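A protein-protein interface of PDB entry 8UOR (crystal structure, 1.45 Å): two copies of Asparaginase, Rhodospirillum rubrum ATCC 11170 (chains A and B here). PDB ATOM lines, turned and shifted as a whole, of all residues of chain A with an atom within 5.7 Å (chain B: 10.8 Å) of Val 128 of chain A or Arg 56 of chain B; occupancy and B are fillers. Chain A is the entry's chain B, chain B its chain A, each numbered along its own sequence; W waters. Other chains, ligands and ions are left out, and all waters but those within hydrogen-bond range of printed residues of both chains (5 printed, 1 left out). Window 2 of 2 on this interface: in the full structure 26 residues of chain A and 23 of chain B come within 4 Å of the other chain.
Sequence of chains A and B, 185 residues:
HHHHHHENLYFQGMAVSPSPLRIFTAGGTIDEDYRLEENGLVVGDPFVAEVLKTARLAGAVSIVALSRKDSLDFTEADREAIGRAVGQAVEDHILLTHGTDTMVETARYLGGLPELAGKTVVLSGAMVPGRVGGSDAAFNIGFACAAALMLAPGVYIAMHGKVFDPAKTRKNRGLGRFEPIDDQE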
ATOM      1  N   THR A  29     -16.702 -15.698 -17.983  1.00  0.00           N
ATOM      2  CA  THR A  29     -16.600 -14.209 -18.056  1.00  0.00           C
ATOM      3  C   THR A  29     -16.439 -13.719 -19.484  1.00  0.00           C
ATOM      4  O   THR A  29     -17.074 -12.738 -19.904  1.00  0.00           O
ATOM      5  CB  THR A  29     -15.457 -13.713 -17.157  1.00  0.00           C
ATOM      6  OG1 THR A  29     -15.647 -14.220 -15.851  1.00  0.00           O
ATOM      7  CG2 THR A  29     -15.369 -12.211 -17.183  1.00  0.00           C
ATOM      8  N   ILE A  30     -15.635 -14.436 -20.276  1.00  0.00           N
ATOM      9  CA  ILE A  30     -15.379 -14.013 -21.655  1.00  0.00           C
ATOM     10  C   ILE A  30     -16.692 -13.717 -22.379  1.00  0.00           C
ATOM     11  O   ILE A  30     -16.739 -12.798 -23.230  1.00  0.00           O
ATOM     12  CB  ILE A  30     -14.513 -15.044 -22.382  1.00  0.00           C
ATOM     13  CG1 ILE A  30     -14.187 -14.543 -23.779  1.00  0.00           C
ATOM     14  CG2 ILE A  30     -15.123 -16.445 -22.397  1.00  0.00           C
ATOM     15  CD1 ILE A  30     -13.069 -15.338 -24.461  1.00  0.00           C
ATOM     16  N   ALA A 126     -11.218 -15.114 -20.484  1.00  0.00           N
ATOM     17  CA  ALA A 126     -10.847 -13.709 -20.285  1.00  0.00           C
ATOM     18  C   ALA A 126     -11.150 -13.352 -18.840  1.00  0.00           C
ATOM     19  O   ALA A 126     -12.110 -13.839 -18.280  1.00  0.00           O
ATOM     20  CB  ALA A 126     -11.620 -12.828 -21.246  1.00  0.00           C
ATOM     21  N   MET A 127     -10.359 -12.395 -18.340  1.00  0.00           N
ATOM     22  CA  MET A 127     -10.649 -11.809 -17.022  1.00  0.00           C
ATOM     23  C   MET A 127     -11.736 -10.731 -17.075  1.00  0.00           C
ATOM     24  O   MET A 127     -12.356 -10.441 -16.079  1.00  0.00           O
ATOM     25  CB  MET A 127      -9.373 -11.213 -16.460  1.00  0.00           C
ATOM     26  CG  MET A 127      -8.202 -12.201 -16.163  1.00  0.00           C
ATOM     27  SD  MET A 127      -8.750 -13.731 -15.352  1.00  0.00           S
ATOM     28  CE  MET A 127      -9.566 -13.131 -13.901  1.00  0.00           C
ATOM     29  N   VAL A 128     -11.907 -10.110 -18.253  1.00  0.00           N
ATOM     30  CA  VAL A 128     -12.913  -9.048 -18.497  1.00  0.00           C
ATOM     31  C   VAL A 128     -13.772  -9.501 -19.665  1.00  0.00           C
ATOM     32  O   VAL A 128     -13.247  -9.978 -20.671  1.00  0.00           O
ATOM     33  CB  VAL A 128     -12.191  -7.734 -18.857  1.00  0.00           C
ATOM     34  CG1 VAL A 128     -13.176  -6.622 -19.250  1.00  0.00           C
ATOM     35  CG2 VAL A 128     -11.291  -7.258 -17.726  1.00  0.00           C
ATOM     36  N   PRO A 129     -15.087  -9.434 -19.565  1.00  0.00           N
ATOM     37  CA  PRO A 129     -15.937  -9.879 -20.677  1.00  0.00           C
ATOM     38  C   PRO A 129     -15.515  -9.237 -21.984  1.00  0.00           C
ATOM     39  O   PRO A 129     -15.231  -8.047 -22.057  1.00  0.00           O
ATOM     40  CB  PRO A 129     -17.328  -9.394 -20.285  1.00  0.00           C
ATOM     41  CG  PRO A 129     -17.305  -9.341 -18.761  1.00  0.00           C
ATOM     42  CD  PRO A 129     -15.905  -8.901 -18.468  1.00  0.00           C
ATOM     43  N   GLY A 130     -15.572  -9.987 -23.070  1.00  0.00           N
ATOM     44  CA  GLY A 130     -15.238  -9.477 -24.409  1.00  0.00           C
ATOM     45  C   GLY A 130     -16.080  -8.259 -24.791  1.00  0.00           C
ATOM     46  O   GLY A 130     -15.581  -7.361 -25.487  1.00  0.00           O
ATOM     47  N   VAL A 132     -17.178  -5.927 -22.811  1.00  0.00           N
ATOM     48  CA  VAL A 132     -16.834  -4.755 -21.993  1.00  0.00           C
ATOM     49  C   VAL A 132     -15.584  -4.115 -22.582  1.00  0.00           C
ATOM     50  O   VAL A 132     -14.624  -4.846 -22.944  1.00  0.00           O
ATOM     51  CB  VAL A 132     -16.646  -5.213 -20.533  1.00  0.00           C
ATOM     52  CG1 VAL A 132     -16.006  -4.138 -19.685  1.00  0.00           C
ATOM     53  CG2 VAL A 132     -17.989  -5.614 -19.957  1.00  0.00           C
ATOM     54  N   GLY A 133     -15.505  -2.783 -22.502  1.00  0.00           N
ATOM     55  CA  GLY A 133     -14.285  -2.121 -23.018  1.00  0.00           C
ATOM     56  C   GLY A 133     -13.028  -2.544 -22.265  1.00  0.00           C
ATOM     57  O   GLY A 133     -13.071  -2.752 -21.051  1.00  0.00           O
ATOM     58  N   GLY A 134     -11.937  -2.606 -23.006  1.00  0.00           N
ATOM     59  CA  GLY A 134     -10.667  -2.939 -22.356  1.00  0.00           C
ATOM     60  C   GLY A 134     -10.439  -4.393 -22.054  1.00  0.00           C
ATOM     61  O   GLY A 134      -9.671  -4.701 -21.145  1.00  0.00           O
ATOM     62  N   SER A 135     -11.177  -5.277 -22.718  1.00  0.00           N
ATOM     63  CA  SER A 135     -11.045  -6.714 -22.465  1.00  0.00           C
ATOM     64  C   SER A 135      -9.767  -7.305 -23.083  1.00  0.00           C
ATOM     65  O   SER A 135      -9.359  -6.966 -24.198  1.00  0.00           O
ATOM     66  CB  SER A 135     -12.266  -7.424 -23.067  1.00  0.00           C
ATOM     67  OG  SER A 135     -12.155  -8.824 -22.873  1.00  0.00           O
ATOM     68  N   ASP A 136      -9.229  -8.295 -22.393  1.00  0.00           N
ATOM     69  CA  ASP A 136      -8.149  -9.201 -22.822  1.00  0.00           C
ATOM     70  C   ASP A 136      -8.653 -10.271 -23.814  1.00  0.00           C
ATOM     71  O   ASP A 136      -7.786 -10.993 -24.349  1.00  0.00           O
ATOM     72  CB  ASP A 136      -7.517  -9.891 -21.578  1.00  0.00           C
ATOM     73  CG  ASP A 136      -8.523 -10.538 -20.560  1.00  0.00           C
ATOM     74  OD1 ASP A 136      -9.656  -9.992 -20.322  1.00  0.00           O
ATOM     75  OD2 ASP A 136      -8.166 -11.558 -19.933  1.00  0.00           O
ATOM     76  N   ALA A 137      -9.952 -10.396 -24.060  1.00  0.00           N
ATOM     77  CA  ALA A 137     -10.476 -11.570 -24.783  1.00  0.00           C
ATOM     78  C   ALA A 137      -9.904 -11.711 -26.190  1.00  0.00           C
ATOM     79  O   ALA A 137      -9.500 -12.832 -26.508  1.00  0.00           O
ATOM     80  CB  ALA A 137     -11.989 -11.446 -24.858  1.00  0.00           C
ATOM     81  N   MET A 159      -3.155 -17.972 -20.994  1.00  0.00           N
ATOM     82  CA  MET A 159      -3.736 -16.745 -20.460  1.00  0.00           C
ATOM     83  C   MET A 159      -2.521 -15.830 -20.154  1.00  0.00           C
ATOM     84  O   MET A 159      -1.385 -16.336 -19.978  1.00  0.00           O
ATOM     85  CB  MET A 159      -4.419 -16.985 -19.105  1.00  0.00           C
ATOM     86  CG  MET A 159      -5.725 -17.707 -19.225  1.00  0.00           C
ATOM     87  SD  MET A 159      -7.000 -16.765 -20.138  1.00  0.00           S
ATOM     88  CE  MET A 159      -7.297 -15.446 -19.010  1.00  0.00           C
ATOM     89  N   HIS A 160      -2.735 -14.512 -20.131  1.00  0.00           N
ATOM     90  CA  HIS A 160      -1.658 -13.574 -19.744  1.00  0.00           C
ATOM     91  C   HIS A 160      -0.487 -13.658 -20.698  1.00  0.00           C
ATOM     92  O   HIS A 160       0.646 -13.295 -20.288  1.00  0.00           O
ATOM     93  CB  HIS A 160      -1.165 -13.785 -18.303  1.00  0.00           C
ATOM     94  CG  HIS A 160      -2.280 -14.030 -17.373  1.00  0.00           C
ATOM     95  ND1 HIS A 160      -3.301 -13.135 -17.186  1.00  0.00           N
ATOM     96  CD2 HIS A 160      -2.487 -15.008 -16.458  1.00  0.00           C
ATOM     97  CE1 HIS A 160      -4.151 -13.629 -16.307  1.00  0.00           C
ATOM     98  NE2 HIS A 160      -3.655 -14.745 -15.822  1.00  0.00           N
ATOM     99  N   GLY A 161      -0.703 -14.041 -21.958  1.00  0.00           N
ATOM    100  CA  GLY A 161       0.396 -14.107 -22.925  1.00  0.00           C
ATOM    101  C   GLY A 161       1.411 -15.188 -22.612  1.00  0.00           C
ATOM    102  O   GLY A 161       2.548 -15.065 -23.061  1.00  0.00           O
ATOM    103  N   GLY A 176      -7.326 -11.870  -9.744  1.00  0.00           N
ATOM    104  CA  GLY A 176      -7.818 -12.086 -11.113  1.00  0.00           C
ATOM    105  C   GLY A 176      -6.681 -12.560 -12.017  1.00  0.00           C
ATOM    106  O   GLY A 176      -6.347 -11.938 -13.054  1.00  0.00           O
ATOM    107  N   SER B  17       9.545 -12.943 -13.374  1.00  0.00           N
ATOM    108  CA  SER B  17       8.860 -13.303 -14.640  1.00  0.00           C
ATOM    109  C   SER B  17       9.768 -12.867 -15.786  1.00  0.00           C
ATOM    110  O   SER B  17      10.238 -11.689 -15.871  1.00  0.00           O
ATOM    111  CB  SER B  17       7.484 -12.647 -14.753  1.00  0.00           C
ATOM    112  OG  SER B  17       6.575 -13.194 -13.812  1.00  0.00           O
ATOM    113  N   VAL B  48      -0.134  -2.141 -31.567  1.00  0.00           N
ATOM    114  CA  VAL B  48       0.237  -3.287 -30.747  1.00  0.00           C
ATOM    115  C   VAL B  48       0.342  -2.848 -29.277  1.00  0.00           C
ATOM    116  O   VAL B  48       0.035  -3.637 -28.363  1.00  0.00           O
ATOM    117  CB  VAL B  48       1.507  -3.951 -31.287  1.00  0.00           C
ATOM    118  CG1 VAL B  48       2.715  -3.016 -31.228  1.00  0.00           C
ATOM    119  CG2 VAL B  48       1.767  -5.279 -30.575  1.00  0.00           C
ATOM    120  N   ALA B  49       0.782  -1.612 -28.993  1.00  0.00           N
ATOM    121  CA  ALA B  49       0.878  -1.141 -27.609  1.00  0.00           C
ATOM    122  C   ALA B  49      -0.487  -1.150 -26.944  1.00  0.00           C
ATOM    123  O   ALA B  49      -0.621  -1.481 -25.792  1.00  0.00           O
ATOM    124  CB  ALA B  49       1.562   0.199 -27.528  1.00  0.00           C
ATOM    125  N   GLU B  50      -1.511  -0.720 -27.681  1.00  0.00           N
ATOM    126  CA  GLU B  50      -2.895  -0.673 -27.172  1.00  0.00           C
ATOM    127  C   GLU B  50      -3.355  -2.065 -26.822  1.00  0.00           C
ATOM    128  O   GLU B  50      -4.058  -2.255 -25.837  1.00  0.00           O
ATOM    129  CB  GLU B  50      -3.813   0.044 -28.140  1.00  0.00           C
ATOM    130  CG  GLU B  50      -3.456   1.454 -28.399  1.00  0.00           C
ATOM    131  CD  GLU B  50      -3.597   2.377 -27.183  1.00  0.00           C
ATOM    132  OE1 GLU B  50      -2.973   3.387 -27.201  1.00  0.00           O
ATOM    133  OE2 GLU B  50      -4.264   2.019 -26.158  1.00  0.00           O
ATOM    134  N   VAL B  51      -3.099  -3.014 -27.711  1.00  0.00           N
ATOM    135  CA  VAL B  51      -3.548  -4.409 -27.484  1.00  0.00           C
ATOM    136  C   VAL B  51      -2.831  -4.962 -26.244  1.00  0.00           C
ATOM    137  O   VAL B  51      -3.456  -5.634 -25.395  1.00  0.00           O
ATOM    138  CB  VAL B  51      -3.299  -5.274 -28.736  1.00  0.00           C
ATOM    139  CG1 VAL B  51      -3.717  -6.697 -28.465  1.00  0.00           C
ATOM    140  CG2 VAL B  51      -4.065  -4.722 -29.951  1.00  0.00           C
ATOM    141  N   LEU B  52      -1.535  -4.745 -26.134  1.00  0.00           N
ATOM    142  CA  LEU B  52      -0.826  -5.382 -24.995  1.00  0.00           C
ATOM    143  C   LEU B  52      -1.173  -4.704 -23.673  1.00  0.00           C
ATOM    144  O   LEU B  52      -1.101  -5.390 -22.671  1.00  0.00           O
ATOM    145  CB  LEU B  52       0.648  -5.428 -25.214  1.00  0.00           C
ATOM    146  CG  LEU B  52       1.160  -6.301 -26.308  1.00  0.00           C
ATOM    147  CD1 LEU B  52       2.601  -6.541 -26.207  1.00  0.00           C
ATOM    148  CD2 LEU B  52       0.433  -7.520 -26.517  1.00  0.00           C
ATOM    149  N   LYS B  53      -1.580  -3.423 -23.706  1.00  0.00           N
ATOM    150  CA  LYS B  53      -1.953  -2.659 -22.503  1.00  0.00           C
ATOM    151  C   LYS B  53      -3.006  -3.408 -21.787  1.00  0.00           C
ATOM    152  O   LYS B  53      -2.946  -3.311 -20.504  1.00  0.00           O
ATOM    153  CB  LYS B  53      -2.396  -1.229 -22.828  1.00  0.00           C
ATOM    154  CG  LYS B  53      -2.809  -0.331 -21.683  1.00  0.00           C
ATOM    155  CD  LYS B  53      -2.920   1.131 -22.080  1.00  0.00           C
ATOM    156  CE  LYS B  53      -2.936   2.050 -20.862  1.00  0.00           C
ATOM    157  NZ  LYS B  53      -3.244   3.475 -21.168  1.00  0.00           N
ATOM    158  N   THR B  54      -3.989  -4.032 -22.493  1.00  0.00           N
ATOM    159  CA  THR B  54      -5.141  -4.657 -21.825  1.00  0.00           C
ATOM    160  C   THR B  54      -5.015  -6.182 -21.815  1.00  0.00           C
ATOM    161  O   THR B  54      -5.970  -6.912 -21.397  1.00  0.00           O
ATOM    162  CB  THR B  54      -6.422  -4.161 -22.474  1.00  0.00           C
ATOM    163  OG1 THR B  54      -6.420  -4.522 -23.881  1.00  0.00           O
ATOM    164  CG2 THR B  54      -6.608  -2.677 -22.302  1.00  0.00           C
ATOM    165  N   ALA B  55      -3.858  -6.733 -22.194  1.00  0.00           N
ATOM    166  CA  ALA B  55      -3.663  -8.209 -22.324  1.00  0.00           C
ATOM    167  C   ALA B  55      -3.389  -8.824 -20.957  1.00  0.00           C
ATOM    168  O   ALA B  55      -3.301 -10.035 -20.864  1.00  0.00           O
ATOM    169  CB  ALA B  55      -2.559  -8.529 -23.300  1.00  0.00           C
ATOM    170  N   ARG B  56      -3.149  -7.987 -19.919  1.00  0.00           N
ATOM    171  CA  ARG B  56      -2.922  -8.516 -18.551  1.00  0.00           C
ATOM    172  C   ARG B  56      -1.741  -9.488 -18.533  1.00  0.00           C
ATOM    173  O   ARG B  56      -1.856 -10.657 -18.017  1.00  0.00           O
ATOM    174  CB  ARG B  56      -4.194  -9.152 -17.970  1.00  0.00           C
ATOM    175  CG  ARG B  56      -5.318  -8.155 -17.946  1.00  0.00           C
ATOM    176  CD  ARG B  56      -6.520  -8.707 -17.261  1.00  0.00           C
ATOM    177  NE  ARG B  56      -7.299  -7.491 -17.168  1.00  0.00           N
ATOM    178  CZ  ARG B  56      -7.576  -6.822 -16.064  1.00  0.00           C
ATOM    179  NH1 ARG B  56      -7.048  -7.101 -14.862  1.00  0.00           N
ATOM    180  NH2 ARG B  56      -8.324  -5.760 -16.230  1.00  0.00           N
ATOM    181  N   LEU B  57      -0.657  -9.070 -19.145  1.00  0.00           N
ATOM    182  CA  LEU B  57       0.480  -9.960 -19.362  1.00  0.00           C
ATOM    183  C   LEU B  57       1.123 -10.372 -18.040  1.00  0.00           C
ATOM    184  O   LEU B  57       1.261  -9.525 -17.113  1.00  0.00           O
ATOM    185  CB  LEU B  57       1.493  -9.260 -20.222  1.00  0.00           C
ATOM    186  CG  LEU B  57       1.054  -8.909 -21.615  1.00  0.00           C
ATOM    187  CD1 LEU B  57       2.157  -8.157 -22.311  1.00  0.00           C
ATOM    188  CD2 LEU B  57       0.660 -10.148 -22.416  1.00  0.00           C
ATOM    189  N   ALA B  58       1.636 -11.594 -18.007  1.00  0.00           N
ATOM    190  CA  ALA B  58       2.437 -12.075 -16.857  1.00  0.00           C
ATOM    191  C   ALA B  58       3.795 -11.414 -16.875  1.00  0.00           C
ATOM    192  O   ALA B  58       4.312 -11.106 -15.762  1.00  0.00           O
ATOM    193  CB  ALA B  58       2.531 -13.588 -16.858  1.00  0.00           C
ATOM    194  N   GLY B  59       4.413 -11.362 -18.037  1.00  0.00           N
ATOM    195  CA  GLY B  59       5.676 -10.680 -18.237  1.00  0.00           C
ATOM    196  C   GLY B  59       5.448  -9.269 -18.741  1.00  0.00           C
ATOM    197  O   GLY B  59       4.473  -8.554 -18.375  1.00  0.00           O
ATOM    198  N   ALA B  60       6.466  -8.744 -19.301  1.00  0.00           N
ATOM    199  CA  ALA B  60       6.397  -7.459 -20.002  1.00  0.00           C
ATOM    200  C   ALA B  60       6.969  -7.637 -21.374  1.00  0.00           C
ATOM    201  O   ALA B  60       7.768  -8.553 -21.625  1.00  0.00           O
ATOM    202  CB  ALA B  60       7.194  -6.474 -19.232  1.00  0.00           C
ATOM    203  N   VAL B  61       6.530  -6.747 -22.221  1.00  0.00           N
ATOM    204  CA  VAL B  61       7.041  -6.739 -23.599  1.00  0.00           C
ATOM    205  C   VAL B  61       7.528  -5.334 -23.895  1.00  0.00           C
ATOM    206  O   VAL B  61       6.739  -4.390 -23.884  1.00  0.00           O
ATOM    207  CB  VAL B  61       5.978  -7.236 -24.607  1.00  0.00           C
ATOM    208  CG1 VAL B  61       6.546  -7.137 -26.020  1.00  0.00           C
ATOM    209  CG2 VAL B  61       5.518  -8.597 -24.292  1.00  0.00           C
ATOM    210  N   ILE B 141      -2.363  -9.879 -33.263  1.00  0.00           N
ATOM    211  CA  ILE B 141      -1.267  -9.653 -32.309  1.00  0.00           C
ATOM    212  C   ILE B 141      -1.198 -10.825 -31.328  1.00  0.00           C
ATOM    213  O   ILE B 141      -0.099 -11.281 -31.026  1.00  0.00           O
ATOM    214  CB  ILE B 141      -1.519  -8.313 -31.609  1.00  0.00           C
ATOM    215  CG1 ILE B 141      -1.310  -7.117 -32.567  1.00  0.00           C
ATOM    216  CG2 ILE B 141      -0.644  -8.221 -30.356  1.00  0.00           C
ATOM    217  CD1 ILE B 141      -0.015  -7.108 -33.339  1.00  0.00           C
HETATM  218  O   HOH W   1      -9.461  -4.511 -25.523  1.00  0.00           O
HETATM  219  O   HOH W   2      -8.014  -6.476 -19.651  1.00  0.00           O
HETATM  220  O   HOH W   3      -5.112  -8.843 -14.051  1.00  0.00           O
HETATM  221  O   HOH W   4      -9.177  -3.964 -18.495  1.00  0.00           O
HETATM  222  O   HOH W   5       3.362 -12.601 -20.587  1.00  0.00           O
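No position is printed for both chains.
The backbone NH (N) of Met 127 of chain A sits at hydrogen-bond distance from the side-chain carboxylate (OD2) of Asp 136 of chain A, 2.8 Å away.
The side-chain hydroxyl (OG) of Ser 135 of chain A is in hydrogen-bond range of the backbone carbonyl oxygen (O) of Val 128 of chain A (2.7 Å).
OD1 of Asp 136 of chain A is in hydrogen-bond range of N of Val 128 of chain A (3.1 Å).
O of Pro 129 of chain A lies close to OG of Ser 135 of chain A.
N of Ala 137 of chain A is in hydrogen-bond range of OG of Ser 135 of chain A (3.0 Å).
Val 128 of chain A touches just one residue of chain B: Arg 56 (3.6 Å).
No residue of chain B comes within 4 Å of Ala 126 of chain A.
Met 127 of chain A touches just one residue of chain B: Arg 56.
No residue of chain B comes within 4 Å of Pro 129 of chain A.
No residue of chain B comes within 4 Å of Gly 130 of chain A.
No residue of chain B comes within 4 Å of Val 132 of chain A.
No residue of chain B comes within 4 Å of Gly 133 of chain A.
Of chain B, only Thr 54 comes within 4 Å of Ser 135 of chain A.
Asp 136 of chain A touches just one residue of chain B: Thr 54.
Of chain B, only Arg 56, Leu 57 and Ala 58 come within 4 Å of His 160 of chain A.
Of the printed residues of chain A, Ala 58 of chain B touches His 160.
Of the printed residues of chain A, Leu 57 of chain B touches His 160.
Of the printed residues of chain A, Thr 54 of chain B touches Gly 134 (3.6 Å), Ser 135 (3.8 Å) and Asp 136 (3.4 Å).
Gly 176 of chain A touches none of the printed residues of chain B.
Gly 59 of chain B touches none of the printed residues of chain A.
The nearest residue of chain B that does not touch Val 128 of chain A is Thr 54 of chain B (6.5 Å).
The nearest residue of chain A that does not touch Arg 56 of chain B is Asp 136 of chain A (4.2 Å).
The nearest printed residue of chain A that does not touch Ala 58 of chain B is Gly 161 of chain A (5.2 Å).
Of the 17 printed residues of chain A, 6 touch a printed residue of chain B.
Printed residues of chain A that touch a printed residue of chain B: Met 127, Val 128, Gly 134, Ser 135, Asp 136 and His 160.
Hydrophobic or aromatic side chains of chain A that line the printed part of chain B: Met 127, Val 128 and His 160.
Along chain A the printed residues that touch a printed residue of chain B span positions 127 to 160.
Printed residues of chain B that touch a printed residue of chain A: Thr 54, Arg 56, Leu 57 and Ala 58.
Hydrophobic or aromatic side chains of chain B that line the printed part of chain A: Leu 57 and Ala 58.
Water W2 lies within hydrogen-bond range of the backbone carbonyl oxygen of Thr 54 of chain B, the guanidinium group of Arg 56 of chain B and the backbone carbonyl oxygen of Gly 134 of chain A.
Water W3 lies within hydrogen-bond range of the guanidinium group (NH1) of Arg 56 of chain B (2.7 Å) and the backbone carbonyl oxygen (O) of Gly 176 of chain A (3.5 Å).
Water W1 lies within hydrogen-bond range of O of Ser 135 of chain A (2.8 Å) and OG1 of Thr 54 of chain B (3.5 Å).
Water W4 bridges O of Gly 134 of chain A and NH2 of Arg 56 of chain B.
Water W5 lies within hydrogen-bond range of the backbone carbonyl oxygen of His 160 of chain A (2.8 Å), the backbone NH of Gly 59 of chain B (3.0 Å) and the backbone NH of Ala 58 of chain B (3.3 Å).
O of Arg 56 of chain B sits at hydrogen-bond distance from ND1 of His 160 of chain A.
The backbone NH (N) of Ala 58 of chain B is in hydrogen-bond range of the backbone carbonyl oxygen (O) of His 160 of chain A.
Among the printed residues, merely in contact across the chains: Met 127 of chain A with Arg 56 of chain B (3.9 Å), Val 128 of chain A with Arg 56 of chain B (3.6 Å), Gly 134 of chain A with Thr 54 of chain B (3.6 Å), Ser 135 of chain A with Thr 54 of chain B (3.8 Å), Asp 136 of chain A with Thr 54 of chain B (3.4 Å) and His 160 of chain A with Leu 57 of chain B (3.5 Å).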
